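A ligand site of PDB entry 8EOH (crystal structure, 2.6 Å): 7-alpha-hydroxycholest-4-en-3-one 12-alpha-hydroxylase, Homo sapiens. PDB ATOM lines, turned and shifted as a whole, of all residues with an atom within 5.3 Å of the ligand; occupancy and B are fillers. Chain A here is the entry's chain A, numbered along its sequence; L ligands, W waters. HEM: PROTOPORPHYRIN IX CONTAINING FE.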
ATOM      1  N   PHE A  81       3.821 -28.645  -4.525  1.00  0.00           N
ATOM      2  CA  PHE A  81       4.043 -27.545  -5.454  1.00  0.00           C
ATOM      3  C   PHE A  81       5.381 -26.854  -5.230  1.00  0.00           C
ATOM      4  O   PHE A  81       6.124 -26.627  -6.183  1.00  0.00           O
ATOM      5  CB  PHE A  81       2.939 -26.503  -5.351  1.00  0.00           C
ATOM      6  CG  PHE A  81       3.075 -25.398  -6.347  1.00  0.00           C
ATOM      7  CD1 PHE A  81       3.310 -24.101  -5.937  1.00  0.00           C
ATOM      8  CD2 PHE A  81       2.977 -25.671  -7.709  1.00  0.00           C
ATOM      9  CE1 PHE A  81       3.444 -23.086  -6.866  1.00  0.00           C
ATOM     10  CE2 PHE A  81       3.103 -24.659  -8.636  1.00  0.00           C
ATOM     11  CZ  PHE A  81       3.341 -23.365  -8.216  1.00  0.00           C
ATOM     12  N   HIS A 102       9.315 -17.932   0.217  1.00  0.00           N
ATOM     13  CA  HIS A 102       7.938 -18.161  -0.202  1.00  0.00           C
ATOM     14  C   HIS A 102       6.977 -17.698   0.888  1.00  0.00           C
ATOM     15  O   HIS A 102       6.113 -16.850   0.657  1.00  0.00           O
ATOM     16  CB  HIS A 102       7.686 -19.636  -0.529  1.00  0.00           C
ATOM     17  CG  HIS A 102       6.232 -19.952  -0.735  1.00  0.00           C
ATOM     18  ND1 HIS A 102       5.303 -19.906   0.281  1.00  0.00           N
ATOM     19  CD2 HIS A 102       5.545 -20.291  -1.852  1.00  0.00           C
ATOM     20  CE1 HIS A 102       4.108 -20.210  -0.197  1.00  0.00           C
ATOM     21  NE2 HIS A 102       4.234 -20.452  -1.499  1.00  0.00           N
ATOM     22  N   ILE A 105       6.508 -14.193   0.804  1.00  0.00           N
ATOM     23  CA  ILE A 105       5.734 -13.652  -0.319  1.00  0.00           C
ATOM     24  C   ILE A 105       4.254 -13.623   0.029  1.00  0.00           C
ATOM     25  O   ILE A 105       3.605 -12.577   0.006  1.00  0.00           O
ATOM     26  CB  ILE A 105       6.006 -14.450  -1.604  1.00  0.00           C
ATOM     27  CG1 ILE A 105       7.381 -14.100  -2.185  1.00  0.00           C
ATOM     28  CG2 ILE A 105       4.917 -14.165  -2.633  1.00  0.00           C
ATOM     29  CD1 ILE A 105       7.691 -14.773  -3.509  1.00  0.00           C
ATOM     30  N   HIS A 106       3.697 -14.798   0.343  1.00  0.00           N
ATOM     31  CA  HIS A 106       2.264 -14.866   0.630  1.00  0.00           C
ATOM     32  C   HIS A 106       1.924 -14.178   1.946  1.00  0.00           C
ATOM     33  O   HIS A 106       0.850 -13.575   2.067  1.00  0.00           O
ATOM     34  CB  HIS A 106       1.806 -16.311   0.631  1.00  0.00           C
ATOM     35  CG  HIS A 106       1.587 -16.887  -0.736  1.00  0.00           C
ATOM     36  ND1 HIS A 106       0.331 -17.120  -1.252  1.00  0.00           N
ATOM     37  CD2 HIS A 106       2.469 -17.243  -1.698  1.00  0.00           C
ATOM     38  CE1 HIS A 106       0.447 -17.613  -2.478  1.00  0.00           C
ATOM     39  NE2 HIS A 106       1.729 -17.693  -2.769  1.00  0.00           N
ATOM     40  N   LEU A 113      -1.645  -6.779   0.009  1.00  0.00           N
ATOM     41  CA  LEU A 113      -2.409  -6.863  -1.218  1.00  0.00           C
ATOM     42  C   LEU A 113      -3.846  -7.302  -0.982  1.00  0.00           C
ATOM     43  O   LEU A 113      -4.513  -7.781  -1.900  1.00  0.00           O
ATOM     44  CB  LEU A 113      -1.727  -7.804  -2.212  1.00  0.00           C
ATOM     45  CG  LEU A 113      -0.366  -7.364  -2.747  1.00  0.00           C
ATOM     46  CD1 LEU A 113       0.053  -8.256  -3.910  1.00  0.00           C
ATOM     47  CD2 LEU A 113      -0.381  -5.895  -3.174  1.00  0.00           C
ATOM     48  N   LEU A 167       3.358  -0.077  -7.579  1.00  0.00           N
ATOM     49  CA  LEU A 167       3.989  -1.139  -6.818  1.00  0.00           C
ATOM     50  C   LEU A 167       5.475  -0.902  -6.575  1.00  0.00           C
ATOM     51  O   LEU A 167       5.959  -1.187  -5.477  1.00  0.00           O
ATOM     52  CB  LEU A 167       3.814  -2.475  -7.540  1.00  0.00           C
ATOM     53  CG  LEU A 167       2.420  -3.091  -7.555  1.00  0.00           C
ATOM     54  CD1 LEU A 167       2.446  -4.454  -8.234  1.00  0.00           C
ATOM     55  CD2 LEU A 167       1.868  -3.226  -6.137  1.00  0.00           C
ATOM     56  N   TRP A 236       4.134  -4.104  -0.096  1.00  0.00           N
ATOM     57  CA  TRP A 236       4.380  -5.425  -0.625  1.00  0.00           C
ATOM     58  C   TRP A 236       5.831  -5.595  -1.006  1.00  0.00           C
ATOM     59  O   TRP A 236       6.518  -6.418  -0.469  1.00  0.00           O
ATOM     60  CB  TRP A 236       3.477  -5.640  -1.823  1.00  0.00           C
ATOM     61  CG  TRP A 236       3.517  -6.981  -2.362  1.00  0.00           C
ATOM     62  CD1 TRP A 236       3.147  -8.093  -1.730  1.00  0.00           C
ATOM     63  CD2 TRP A 236       3.888  -7.362  -3.672  1.00  0.00           C
ATOM     64  NE1 TRP A 236       3.272  -9.165  -2.550  1.00  0.00           N
ATOM     65  CE2 TRP A 236       3.732  -8.733  -3.759  1.00  0.00           C
ATOM     66  CE3 TRP A 236       4.360  -6.676  -4.772  1.00  0.00           C
ATOM     67  CZ2 TRP A 236       4.022  -9.431  -4.898  1.00  0.00           C
ATOM     68  CZ3 TRP A 236       4.641  -7.371  -5.896  1.00  0.00           C
ATOM     69  CH2 TRP A 236       4.477  -8.732  -5.957  1.00  0.00           C
ATOM     70  N   MET A 261       9.102 -10.410  -9.790  1.00  0.00           N
ATOM     71  CA  MET A 261       7.855  -9.835  -9.300  1.00  0.00           C
ATOM     72  C   MET A 261       7.233  -8.916 -10.347  1.00  0.00           C
ATOM     73  O   MET A 261       6.002  -8.872 -10.483  1.00  0.00           O
ATOM     74  CB  MET A 261       8.096  -9.085  -7.999  1.00  0.00           C
ATOM     75  CG  MET A 261       8.338  -9.990  -6.807  1.00  0.00           C
ATOM     76  SD  MET A 261       6.996 -11.160  -6.511  1.00  0.00           S
ATOM     77  CE  MET A 261       7.841 -12.723  -6.731  1.00  0.00           C
ATOM     78  N   ALA A 264       5.387 -11.160 -12.658  1.00  0.00           N
ATOM     79  CA  ALA A 264       4.160 -11.712 -12.087  1.00  0.00           C
ATOM     80  C   ALA A 264       3.070 -10.660 -11.998  1.00  0.00           C
ATOM     81  O   ALA A 264       1.900 -10.934 -12.282  1.00  0.00           O
ATOM     82  CB  ALA A 264       4.453 -12.316 -10.725  1.00  0.00           C
ATOM     83  N   SER A 265       3.422  -9.435 -11.590  1.00  0.00           N
ATOM     84  CA  SER A 265       2.409  -8.441 -11.291  1.00  0.00           C
ATOM     85  C   SER A 265       1.874  -7.745 -12.538  1.00  0.00           C
ATOM     86  O   SER A 265       0.721  -7.301 -12.545  1.00  0.00           O
ATOM     87  CB  SER A 265       2.960  -7.401 -10.313  1.00  0.00           C
ATOM     88  OG  SER A 265       3.915  -6.575 -10.942  1.00  0.00           O
ATOM     89  N   ASN A 268      -0.059 -10.251 -16.720  1.00  0.00           N
ATOM     90  CA  ASN A 268      -1.414 -10.682 -17.074  1.00  0.00           C
ATOM     91  C   ASN A 268      -2.476  -9.609 -16.925  1.00  0.00           C
ATOM     92  O   ASN A 268      -3.515  -9.701 -17.582  1.00  0.00           O
ATOM     93  CB  ASN A 268      -1.831 -11.889 -16.210  1.00  0.00           C
ATOM     94  CG  ASN A 268      -1.005 -13.125 -16.499  1.00  0.00           C
ATOM     95  OD1 ASN A 268      -1.239 -13.828 -17.478  1.00  0.00           O
ATOM     96  ND2 ASN A 268      -0.037 -13.405 -15.632  1.00  0.00           N
ATOM     97  N   THR A 269      -2.265  -8.603 -16.074  1.00  0.00           N
ATOM     98  CA  THR A 269      -3.307  -7.607 -15.841  1.00  0.00           C
ATOM     99  C   THR A 269      -3.675  -6.894 -17.142  1.00  0.00           C
ATOM    100  O   THR A 269      -4.855  -6.812 -17.504  1.00  0.00           O
ATOM    101  CB  THR A 269      -2.848  -6.599 -14.794  1.00  0.00           C
ATOM    102  OG1 THR A 269      -2.296  -7.294 -13.662  1.00  0.00           O
ATOM    103  CG2 THR A 269      -4.008  -5.741 -14.335  1.00  0.00           C
ATOM    104  N   THR A 272      -5.508  -9.061 -19.764  1.00  0.00           N
ATOM    105  CA  THR A 272      -6.877  -9.281 -19.296  1.00  0.00           C
ATOM    106  C   THR A 272      -7.755  -8.069 -19.601  1.00  0.00           C
ATOM    107  O   THR A 272      -8.840  -8.207 -20.166  1.00  0.00           O
ATOM    108  CB  THR A 272      -6.876  -9.575 -17.793  1.00  0.00           C
ATOM    109  OG1 THR A 272      -6.210 -10.816 -17.540  1.00  0.00           O
ATOM    110  CG2 THR A 272      -8.306  -9.636 -17.267  1.00  0.00           C
ATOM    111  N   LEU A 330     -12.080 -13.860 -17.738  1.00  0.00           N
ATOM    112  CA  LEU A 330     -11.066 -14.787 -17.263  1.00  0.00           C
ATOM    113  C   LEU A 330     -11.377 -16.211 -17.698  1.00  0.00           C
ATOM    114  O   LEU A 330     -10.490 -16.956 -18.134  1.00  0.00           O
ATOM    115  CB  LEU A 330     -10.947 -14.707 -15.737  1.00  0.00           C
ATOM    116  CG  LEU A 330     -10.558 -13.337 -15.168  1.00  0.00           C
ATOM    117  CD1 LEU A 330     -10.460 -13.396 -13.644  1.00  0.00           C
ATOM    118  CD2 LEU A 330      -9.253 -12.859 -15.771  1.00  0.00           C
ATOM    119  N   PRO A 336      -4.029 -20.979 -17.478  1.00  0.00           N
ATOM    120  CA  PRO A 336      -2.807 -21.496 -16.873  1.00  0.00           C
ATOM    121  C   PRO A 336      -2.868 -23.013 -16.734  1.00  0.00           C
ATOM    122  O   PRO A 336      -3.884 -23.657 -17.017  1.00  0.00           O
ATOM    123  CB  PRO A 336      -2.767 -20.812 -15.506  1.00  0.00           C
ATOM    124  CG  PRO A 336      -4.228 -20.619 -15.171  1.00  0.00           C
ATOM    125  CD  PRO A 336      -4.898 -20.310 -16.481  1.00  0.00           C
ATOM    126  N   LEU A 338      -2.119 -26.066 -13.925  1.00  0.00           N
ATOM    127  CA  LEU A 338      -1.828 -26.435 -12.541  1.00  0.00           C
ATOM    128  C   LEU A 338      -0.877 -27.623 -12.526  1.00  0.00           C
ATOM    129  O   LEU A 338      -1.150 -28.644 -13.164  1.00  0.00           O
ATOM    130  CB  LEU A 338      -3.121 -26.772 -11.789  1.00  0.00           C
ATOM    131  CG  LEU A 338      -3.862 -25.591 -11.164  1.00  0.00           C
ATOM    132  CD1 LEU A 338      -3.151 -25.116  -9.904  1.00  0.00           C
ATOM    133  CD2 LEU A 338      -4.015 -24.458 -12.161  1.00  0.00           C
ATOM    134  N   ARG A 340       1.746 -30.234 -10.191  1.00  0.00           N
ATOM    135  CA  ARG A 340       2.039 -30.817  -8.889  1.00  0.00           C
ATOM    136  C   ARG A 340       3.039 -31.947  -9.062  1.00  0.00           C
ATOM    137  O   ARG A 340       2.788 -32.866  -9.846  1.00  0.00           O
ATOM    138  CB  ARG A 340       0.771 -31.342  -8.211  1.00  0.00           C
ATOM    139  CG  ARG A 340      -0.312 -30.318  -7.968  1.00  0.00           C
ATOM    140  CD  ARG A 340       0.112 -29.259  -6.973  1.00  0.00           C
ATOM    141  NE  ARG A 340      -1.028 -28.465  -6.536  1.00  0.00           N
ATOM    142  CZ  ARG A 340      -1.367 -27.290  -7.058  1.00  0.00           C
ATOM    143  NH1 ARG A 340      -0.658 -26.756  -8.038  1.00  0.00           N
ATOM    144  NH2 ARG A 340      -2.428 -26.645  -6.596  1.00  0.00           N
ATOM    145  N   PRO A 414      -8.621 -19.176 -12.913  1.00  0.00           N
ATOM    146  CA  PRO A 414      -7.633 -18.302 -13.554  1.00  0.00           C
ATOM    147  C   PRO A 414      -6.465 -17.942 -12.653  1.00  0.00           C
ATOM    148  O   PRO A 414      -5.477 -17.375 -13.137  1.00  0.00           O
ATOM    149  CB  PRO A 414      -8.448 -17.053 -13.905  1.00  0.00           C
ATOM    150  CG  PRO A 414      -9.511 -16.995 -12.829  1.00  0.00           C
ATOM    151  CD  PRO A 414      -9.761 -18.420 -12.365  1.00  0.00           C
ATOM    152  N   TRP A 415      -6.543 -18.247 -11.352  1.00  0.00           N
ATOM    153  CA  TRP A 415      -5.507 -17.890 -10.406  1.00  0.00           C
ATOM    154  C   TRP A 415      -4.698 -19.076  -9.887  1.00  0.00           C
ATOM    155  O   TRP A 415      -3.621 -18.856  -9.312  1.00  0.00           O
ATOM    156  CB  TRP A 415      -6.115 -17.179  -9.187  1.00  0.00           C
ATOM    157  CG  TRP A 415      -7.187 -16.187  -9.519  1.00  0.00           C
ATOM    158  CD1 TRP A 415      -8.528 -16.347  -9.328  1.00  0.00           C
ATOM    159  CD2 TRP A 415      -7.012 -14.892 -10.095  1.00  0.00           C
ATOM    160  NE1 TRP A 415      -9.197 -15.227  -9.748  1.00  0.00           N
ATOM    161  CE2 TRP A 415      -8.293 -14.316 -10.221  1.00  0.00           C
ATOM    162  CE3 TRP A 415      -5.898 -14.155 -10.507  1.00  0.00           C
ATOM    163  CZ2 TRP A 415      -8.485 -13.046 -10.752  1.00  0.00           C
ATOM    164  CZ3 TRP A 415      -6.093 -12.900 -11.029  1.00  0.00           C
ATOM    165  CH2 TRP A 415      -7.383 -12.351 -11.148  1.00  0.00           C
ATOM    166  N   GLY A 416      -5.181 -20.301 -10.066  1.00  0.00           N
ATOM    167  CA  GLY A 416      -4.523 -21.458  -9.487  1.00  0.00           C
ATOM    168  C   GLY A 416      -5.289 -22.002  -8.306  1.00  0.00           C
ATOM    169  O   GLY A 416      -6.506 -21.831  -8.223  1.00  0.00           O
ATOM    170  N   SER A 417      -4.586 -22.662  -7.391  1.00  0.00           N
ATOM    171  CA  SER A 417      -5.230 -23.194  -6.195  1.00  0.00           C
ATOM    172  C   SER A 417      -4.156 -23.550  -5.166  1.00  0.00           C
ATOM    173  O   SER A 417      -2.972 -23.659  -5.494  1.00  0.00           O
ATOM    174  CB  SER A 417      -6.096 -24.409  -6.509  1.00  0.00           C
ATOM    175  OG  SER A 417      -7.211 -24.056  -7.308  1.00  0.00           O
ATOM    176  N   VAL A 419      -1.485 -23.159  -2.311  1.00  0.00           N
ATOM    177  CA  VAL A 419      -0.529 -22.112  -2.002  1.00  0.00           C
ATOM    178  C   VAL A 419       0.223 -21.689  -3.260  1.00  0.00           C
ATOM    179  O   VAL A 419       1.250 -21.013  -3.191  1.00  0.00           O
ATOM    180  CB  VAL A 419       0.459 -22.542  -0.905  1.00  0.00           C
ATOM    181  CG1 VAL A 419      -0.261 -22.671   0.431  1.00  0.00           C
ATOM    182  CG2 VAL A 419       1.117 -23.856  -1.284  1.00  0.00           C
ATOM    183  N   SER A 420      -0.284 -22.094  -4.433  1.00  0.00           N
ATOM    184  CA  SER A 420       0.187 -21.562  -5.699  1.00  0.00           C
ATOM    185  C   SER A 420      -0.698 -20.427  -6.204  1.00  0.00           C
ATOM    186  O   SER A 420      -0.297 -19.696  -7.117  1.00  0.00           O
ATOM    187  CB  SER A 420       0.253 -22.668  -6.766  1.00  0.00           C
ATOM    188  OG  SER A 420      -1.002 -23.326  -6.915  1.00  0.00           O
ATOM    189  N   ILE A 421      -1.882 -20.257  -5.601  1.00  0.00           N
ATOM    190  CA  ILE A 421      -2.842 -19.270  -6.070  1.00  0.00           C
ATOM    191  C   ILE A 421      -2.227 -17.884  -6.074  1.00  0.00           C
ATOM    192  O   ILE A 421      -1.535 -17.474  -5.127  1.00  0.00           O
ATOM    193  CB  ILE A 421      -4.096 -19.321  -5.181  1.00  0.00           C
ATOM    194  CG1 ILE A 421      -5.289 -18.642  -5.845  1.00  0.00           C
ATOM    195  CG2 ILE A 421      -3.806 -18.708  -3.819  1.00  0.00           C
ATOM    196  CD1 ILE A 421      -6.630 -19.152  -5.345  1.00  0.00           C
ATOM    197  N   CYS A 422      -2.481 -17.145  -7.149  1.00  0.00           N
ATOM    198  CA  CYS A 422      -2.041 -15.762  -7.277  1.00  0.00           C
ATOM    199  C   CYS A 422      -2.383 -14.952  -6.030  1.00  0.00           C
ATOM    200  O   CYS A 422      -3.569 -14.672  -5.781  1.00  0.00           O
ATOM    201  CB  CYS A 422      -2.675 -15.139  -8.506  1.00  0.00           C
ATOM    202  SG  CYS A 422      -2.306 -13.419  -8.716  1.00  0.00           S
ATOM    203  N   PRO A 423      -1.392 -14.548  -5.231  1.00  0.00           N
ATOM    204  CA  PRO A 423      -1.687 -13.749  -4.035  1.00  0.00           C
ATOM    205  C   PRO A 423      -1.985 -12.288  -4.322  1.00  0.00           C
ATOM    206  O   PRO A 423      -2.258 -11.537  -3.383  1.00  0.00           O
ATOM    207  CB  PRO A 423      -0.403 -13.902  -3.205  1.00  0.00           C
ATOM    208  CG  PRO A 423       0.677 -14.073  -4.226  1.00  0.00           C
ATOM    209  CD  PRO A 423       0.055 -14.792  -5.399  1.00  0.00           C
ATOM    210  N   GLY A 424      -1.945 -11.865  -5.582  1.00  0.00           N
ATOM    211  CA  GLY A 424      -2.287 -10.503  -5.941  1.00  0.00           C
ATOM    212  C   GLY A 424      -3.556 -10.436  -6.763  1.00  0.00           C
ATOM    213  O   GLY A 424      -3.826  -9.441  -7.438  1.00  0.00           O
ATOM    214  N   ARG A 425      -4.357 -11.502  -6.708  1.00  0.00           N
ATOM    215  CA  ARG A 425      -5.559 -11.569  -7.530  1.00  0.00           C
ATOM    216  C   ARG A 425      -6.547 -10.458  -7.159  1.00  0.00           C
ATOM    217  O   ARG A 425      -7.147  -9.842  -8.044  1.00  0.00           O
ATOM    218  CB  ARG A 425      -6.223 -12.941  -7.386  1.00  0.00           C
ATOM    219  CG  ARG A 425      -6.561 -13.375  -5.960  1.00  0.00           C
ATOM    220  CD  ARG A 425      -7.068 -14.819  -5.975  1.00  0.00           C
ATOM    221  NE  ARG A 425      -7.693 -15.230  -4.725  1.00  0.00           N
ATOM    222  CZ  ARG A 425      -7.037 -15.612  -3.632  1.00  0.00           C
ATOM    223  NH1 ARG A 425      -5.708 -15.631  -3.633  1.00  0.00           N
ATOM    224  NH2 ARG A 425      -7.702 -15.971  -2.541  1.00  0.00           N
ATOM    225  N   PHE A 427      -5.858  -7.563  -5.943  1.00  0.00           N
ATOM    226  CA  PHE A 427      -5.345  -6.328  -6.510  1.00  0.00           C
ATOM    227  C   PHE A 427      -5.554  -6.287  -8.020  1.00  0.00           C
ATOM    228  O   PHE A 427      -6.063  -5.306  -8.560  1.00  0.00           O
ATOM    229  CB  PHE A 427      -3.872  -6.145  -6.188  1.00  0.00           C
ATOM    230  CG  PHE A 427      -3.289  -4.874  -6.728  1.00  0.00           C
ATOM    231  CD1 PHE A 427      -3.964  -3.671  -6.553  1.00  0.00           C
ATOM    232  CD2 PHE A 427      -2.088  -4.866  -7.414  1.00  0.00           C
ATOM    233  CE1 PHE A 427      -3.444  -2.491  -7.048  1.00  0.00           C
ATOM    234  CE2 PHE A 427      -1.565  -3.694  -7.912  1.00  0.00           C
ATOM    235  CZ  PHE A 427      -2.242  -2.507  -7.729  1.00  0.00           C
ATOM    236  N   ALA A 428      -5.170  -7.366  -8.704  1.00  0.00           N
ATOM    237  CA  ALA A 428      -5.345  -7.424 -10.152  1.00  0.00           C
ATOM    238  C   ALA A 428      -6.786  -7.108 -10.543  1.00  0.00           C
ATOM    239  O   ALA A 428      -7.029  -6.389 -11.517  1.00  0.00           O
ATOM    240  CB  ALA A 428      -4.934  -8.793 -10.674  1.00  0.00           C
ATOM    241  N   GLU A 431      -7.333  -3.469 -10.319  1.00  0.00           N
ATOM    242  CA  GLU A 431      -6.732  -2.801 -11.468  1.00  0.00           C
ATOM    243  C   GLU A 431      -7.641  -2.879 -12.687  1.00  0.00           C
ATOM    244  O   GLU A 431      -7.872  -1.871 -13.361  1.00  0.00           O
ATOM    245  CB  GLU A 431      -5.373  -3.433 -11.783  1.00  0.00           C
ATOM    246  CG  GLU A 431      -4.287  -3.200 -10.752  1.00  0.00           C
ATOM    247  CD  GLU A 431      -2.898  -3.549 -11.282  1.00  0.00           C
ATOM    248  OE1 GLU A 431      -2.288  -2.697 -11.960  1.00  0.00           O
ATOM    249  OE2 GLU A 431      -2.432  -4.688 -11.034  1.00  0.00           O
ATOM    250  N   VAL A 432      -8.148  -4.069 -12.990  1.00  0.00           N
ATOM    251  CA  VAL A 432      -8.903  -4.258 -14.222  1.00  0.00           C
ATOM    252  C   VAL A 432     -10.247  -3.540 -14.143  1.00  0.00           C
ATOM    253  O   VAL A 432     -10.649  -2.842 -15.078  1.00  0.00           O
ATOM    254  CB  VAL A 432      -9.091  -5.765 -14.525  1.00  0.00           C
ATOM    255  CG1 VAL A 432     -10.082  -5.966 -15.656  1.00  0.00           C
ATOM    256  CG2 VAL A 432      -7.750  -6.394 -14.864  1.00  0.00           C
ATOM    257  N   GLY A 465      -0.877 -18.428 -18.334  1.00  0.00           N
ATOM    258  CA  GLY A 465      -1.658 -17.350 -17.772  1.00  0.00           C
ATOM    259  C   GLY A 465      -2.744 -16.810 -18.636  1.00  0.00           C
ATOM    260  O   GLY A 465      -3.529 -17.550 -19.129  1.00  0.00           O
ATOM    261  N   THR A 466      -2.810 -15.507 -18.790  1.00  0.00           N
ATOM    262  CA  THR A 466      -3.814 -14.896 -19.656  1.00  0.00           C
ATOM    263  C   THR A 466      -3.323 -14.871 -21.099  1.00  0.00           C
ATOM    264  O   THR A 466      -2.195 -14.463 -21.376  1.00  0.00           O
ATOM    265  CB  THR A 466      -4.140 -13.478 -19.196  1.00  0.00           C
ATOM    266  OG1 THR A 466      -4.728 -13.512 -17.883  1.00  0.00           O
ATOM    267  CG2 THR A 466      -5.116 -12.811 -20.166  1.00  0.00           C
HETATM  268  CHA HEM L   1       0.949 -16.522  -9.573  1.00  0.00           C
HETATM  269  CHB HEM L   1      -2.547 -15.220 -12.663  1.00  0.00           C
HETATM  270  CHC HEM L   1      -2.018 -10.568 -11.271  1.00  0.00           C
HETATM  271  CHD HEM L   1       1.475 -11.898  -8.197  1.00  0.00           C
HETATM  272  C1A HEM L   1      -0.045 -16.546 -10.512  1.00  0.00           C
HETATM  273  C2A HEM L   1      -0.528 -17.719 -11.133  1.00  0.00           C
HETATM  274  C3A HEM L   1      -1.508 -17.355 -11.998  1.00  0.00           C
HETATM  275  C4A HEM L   1      -1.643 -15.964 -11.924  1.00  0.00           C
HETATM  276  CMA HEM L   1      -2.308 -18.292 -12.867  1.00  0.00           C
HETATM  277  CAA HEM L   1      -0.037 -19.122 -10.867  1.00  0.00           C
HETATM  278  CBA HEM L   1      -1.148 -19.924 -10.199  1.00  0.00           C
HETATM  279  CGA HEM L   1      -0.622 -21.295  -9.830  1.00  0.00           C
HETATM  280  O1A HEM L   1      -1.414 -22.190  -9.457  1.00  0.00           O
HETATM  281  O2A HEM L   1       0.601 -21.525  -9.896  1.00  0.00           O
HETATM  282  C1B HEM L   1      -2.668 -13.840 -12.511  1.00  0.00           C
HETATM  283  C2B HEM L   1      -3.621 -13.096 -13.265  1.00  0.00           C
HETATM  284  C3B HEM L   1      -3.499 -11.798 -12.901  1.00  0.00           C
HETATM  285  C4B HEM L   1      -2.425 -11.754 -11.878  1.00  0.00           C
HETATM  286  CMB HEM L   1      -4.581 -13.657 -14.285  1.00  0.00           C
HETATM  287  CAB HEM L   1      -4.273 -10.645 -13.419  1.00  0.00           C
HETATM  288  CBB HEM L   1      -5.203 -10.842 -14.343  1.00  0.00           C
HETATM  289  C1C HEM L   1      -1.036 -10.524 -10.302  1.00  0.00           C
HETATM  290  C2C HEM L   1      -0.617  -9.371  -9.620  1.00  0.00           C
HETATM  291  C3C HEM L   1       0.384  -9.754  -8.745  1.00  0.00           C
HETATM  292  C4C HEM L   1       0.568 -11.156  -8.903  1.00  0.00           C
HETATM  293  CMC HEM L   1      -1.155  -7.975  -9.816  1.00  0.00           C
HETATM  294  CAC HEM L   1       1.109  -8.872  -7.819  1.00  0.00           C
HETATM  295  CBC HEM L   1       0.839  -7.571  -7.773  1.00  0.00           C
HETATM  296  C1D HEM L   1       1.574 -13.283  -8.354  1.00  0.00           C
HETATM  297  C2D HEM L   1       2.546 -14.054  -7.569  1.00  0.00           C
HETATM  298  C3D HEM L   1       2.400 -15.331  -7.952  1.00  0.00           C
HETATM  299  C4D HEM L   1       1.347 -15.339  -8.963  1.00  0.00           C
HETATM  300  CMD HEM L   1       3.509 -13.519  -6.535  1.00  0.00           C
HETATM  301  CAD HEM L   1       3.167 -16.521  -7.430  1.00  0.00           C
HETATM  302  CBD HEM L   1       2.404 -17.174  -6.285  1.00  0.00           C
HETATM  303  CGD HEM L   1       3.325 -18.054  -5.486  1.00  0.00           C
HETATM  304  O1D HEM L   1       2.901 -19.116  -4.987  1.00  0.00           O
HETATM  305  O2D HEM L   1       4.529 -17.733  -5.343  1.00  0.00           O
HETATM  306  NA  HEM L   1      -0.734 -15.465 -11.031  1.00  0.00           N
HETATM  307  NB  HEM L   1      -1.994 -13.013 -11.699  1.00  0.00           N
HETATM  308  NC  HEM L   1      -0.288 -11.589  -9.874  1.00  0.00           N
HETATM  309  ND  HEM L   1       0.882 -14.094  -9.166  1.00  0.00           N
HETATM  310 FE   HEM L   1      -0.464 -13.613 -10.365  1.00  0.00          FE
HETATM  311  O   HOH W   1       1.966 -14.419 -12.574  1.00  0.00           O
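An oxygen (O1D) of the ligand sits close to the backbone carbonyl oxygen (O) of Val 419 (3.1 Å). The side-chain hydroxyl (OG) of Ser 420 sits at hydrogen-bond distance from an oxygen (O1A) of the ligand (2.8 Å). An oxygen (O1D) of the ligand sits at hydrogen-bond distance from a ring nitrogen (NE2) of His 106, at 2.9 Å. An iron atom (FE) of the ligand is bound by the side-chain sulfur (SG) of Cys 422 (2.5 Å).
The backbone carbonyl oxygen (O) of Ser 417 is in hydrogen-bond range of the guanidinium group (NH2) of Arg 340, at 3.2 Å. O of Cys 422 lies within hydrogen-bond range of NH1 of Arg 425 (3.2 Å). The backbone carbonyl oxygen (O) of Ser 417 sits at hydrogen-bond distance from the side-chain hydroxyl (OG) of Ser 420 (2.5 Å). The side-chain hydroxyl (OG1) of Thr 272 sits at hydrogen-bond distance from the backbone carbonyl oxygen (O) of Asn 268 (2.9 Å). The side-chain hydroxyl (OG) of Ser 265 is in hydrogen-bond range of the backbone carbonyl oxygen (O) of Met 261 (3.1 Å). SG of Cys 422 sits close to N of Gly 424, at 3.5 Å. O of Ser 265 lies within hydrogen-bond range of OG1 of Thr 269, at 3.2 Å. OG1 of Thr 466 lies within hydrogen-bond range of OG1 of Thr 272, at 3.1 Å.
The backbone carbonyl oxygen (O) of Ala 264 lies close to a nitrogen (NC) of the ligand (3.3 Å). Merely in contact with the ligand: Phe 81 (3.7 Å), His 102 (3.97 Å), Leu 167 (3.5 Å), Trp 236 (3.9 Å), Ser 265 (3.3 Å), Asn 268 (3.7 Å), Thr 269 (3.9 Å), Thr 272 (3.4 Å), Pro 336 (3.7 Å), Leu 338 (3.4 Å), Pro 414 (3.3 Å), Trp 415 (2.8 Å), Gly 416 (3.2 Å), Ser 417 (3.8 Å), Pro 423 (3.4 Å), Gly 424 (3.9 Å), Ala 428 (3.4 Å), Glu 431 (3.7 Å) and Thr 466 (3.6 Å). Within 4 Å of the ligand: Phe 81, His 102, His 106, Leu 167, Trp 236, Ala 264, Ser 265, Asn 268, Thr 269, Thr 272, Pro 336, Leu 338, Pro 414, Trp 415, Gly 416, Ser 417, Val 419, Ser 420, Cys 422, Pro 423, Gly 424, Ala 428, Glu 431 and Thr 466. The nearest printed residue that does not touch the ligand is Leu 113 (4.001 Å).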
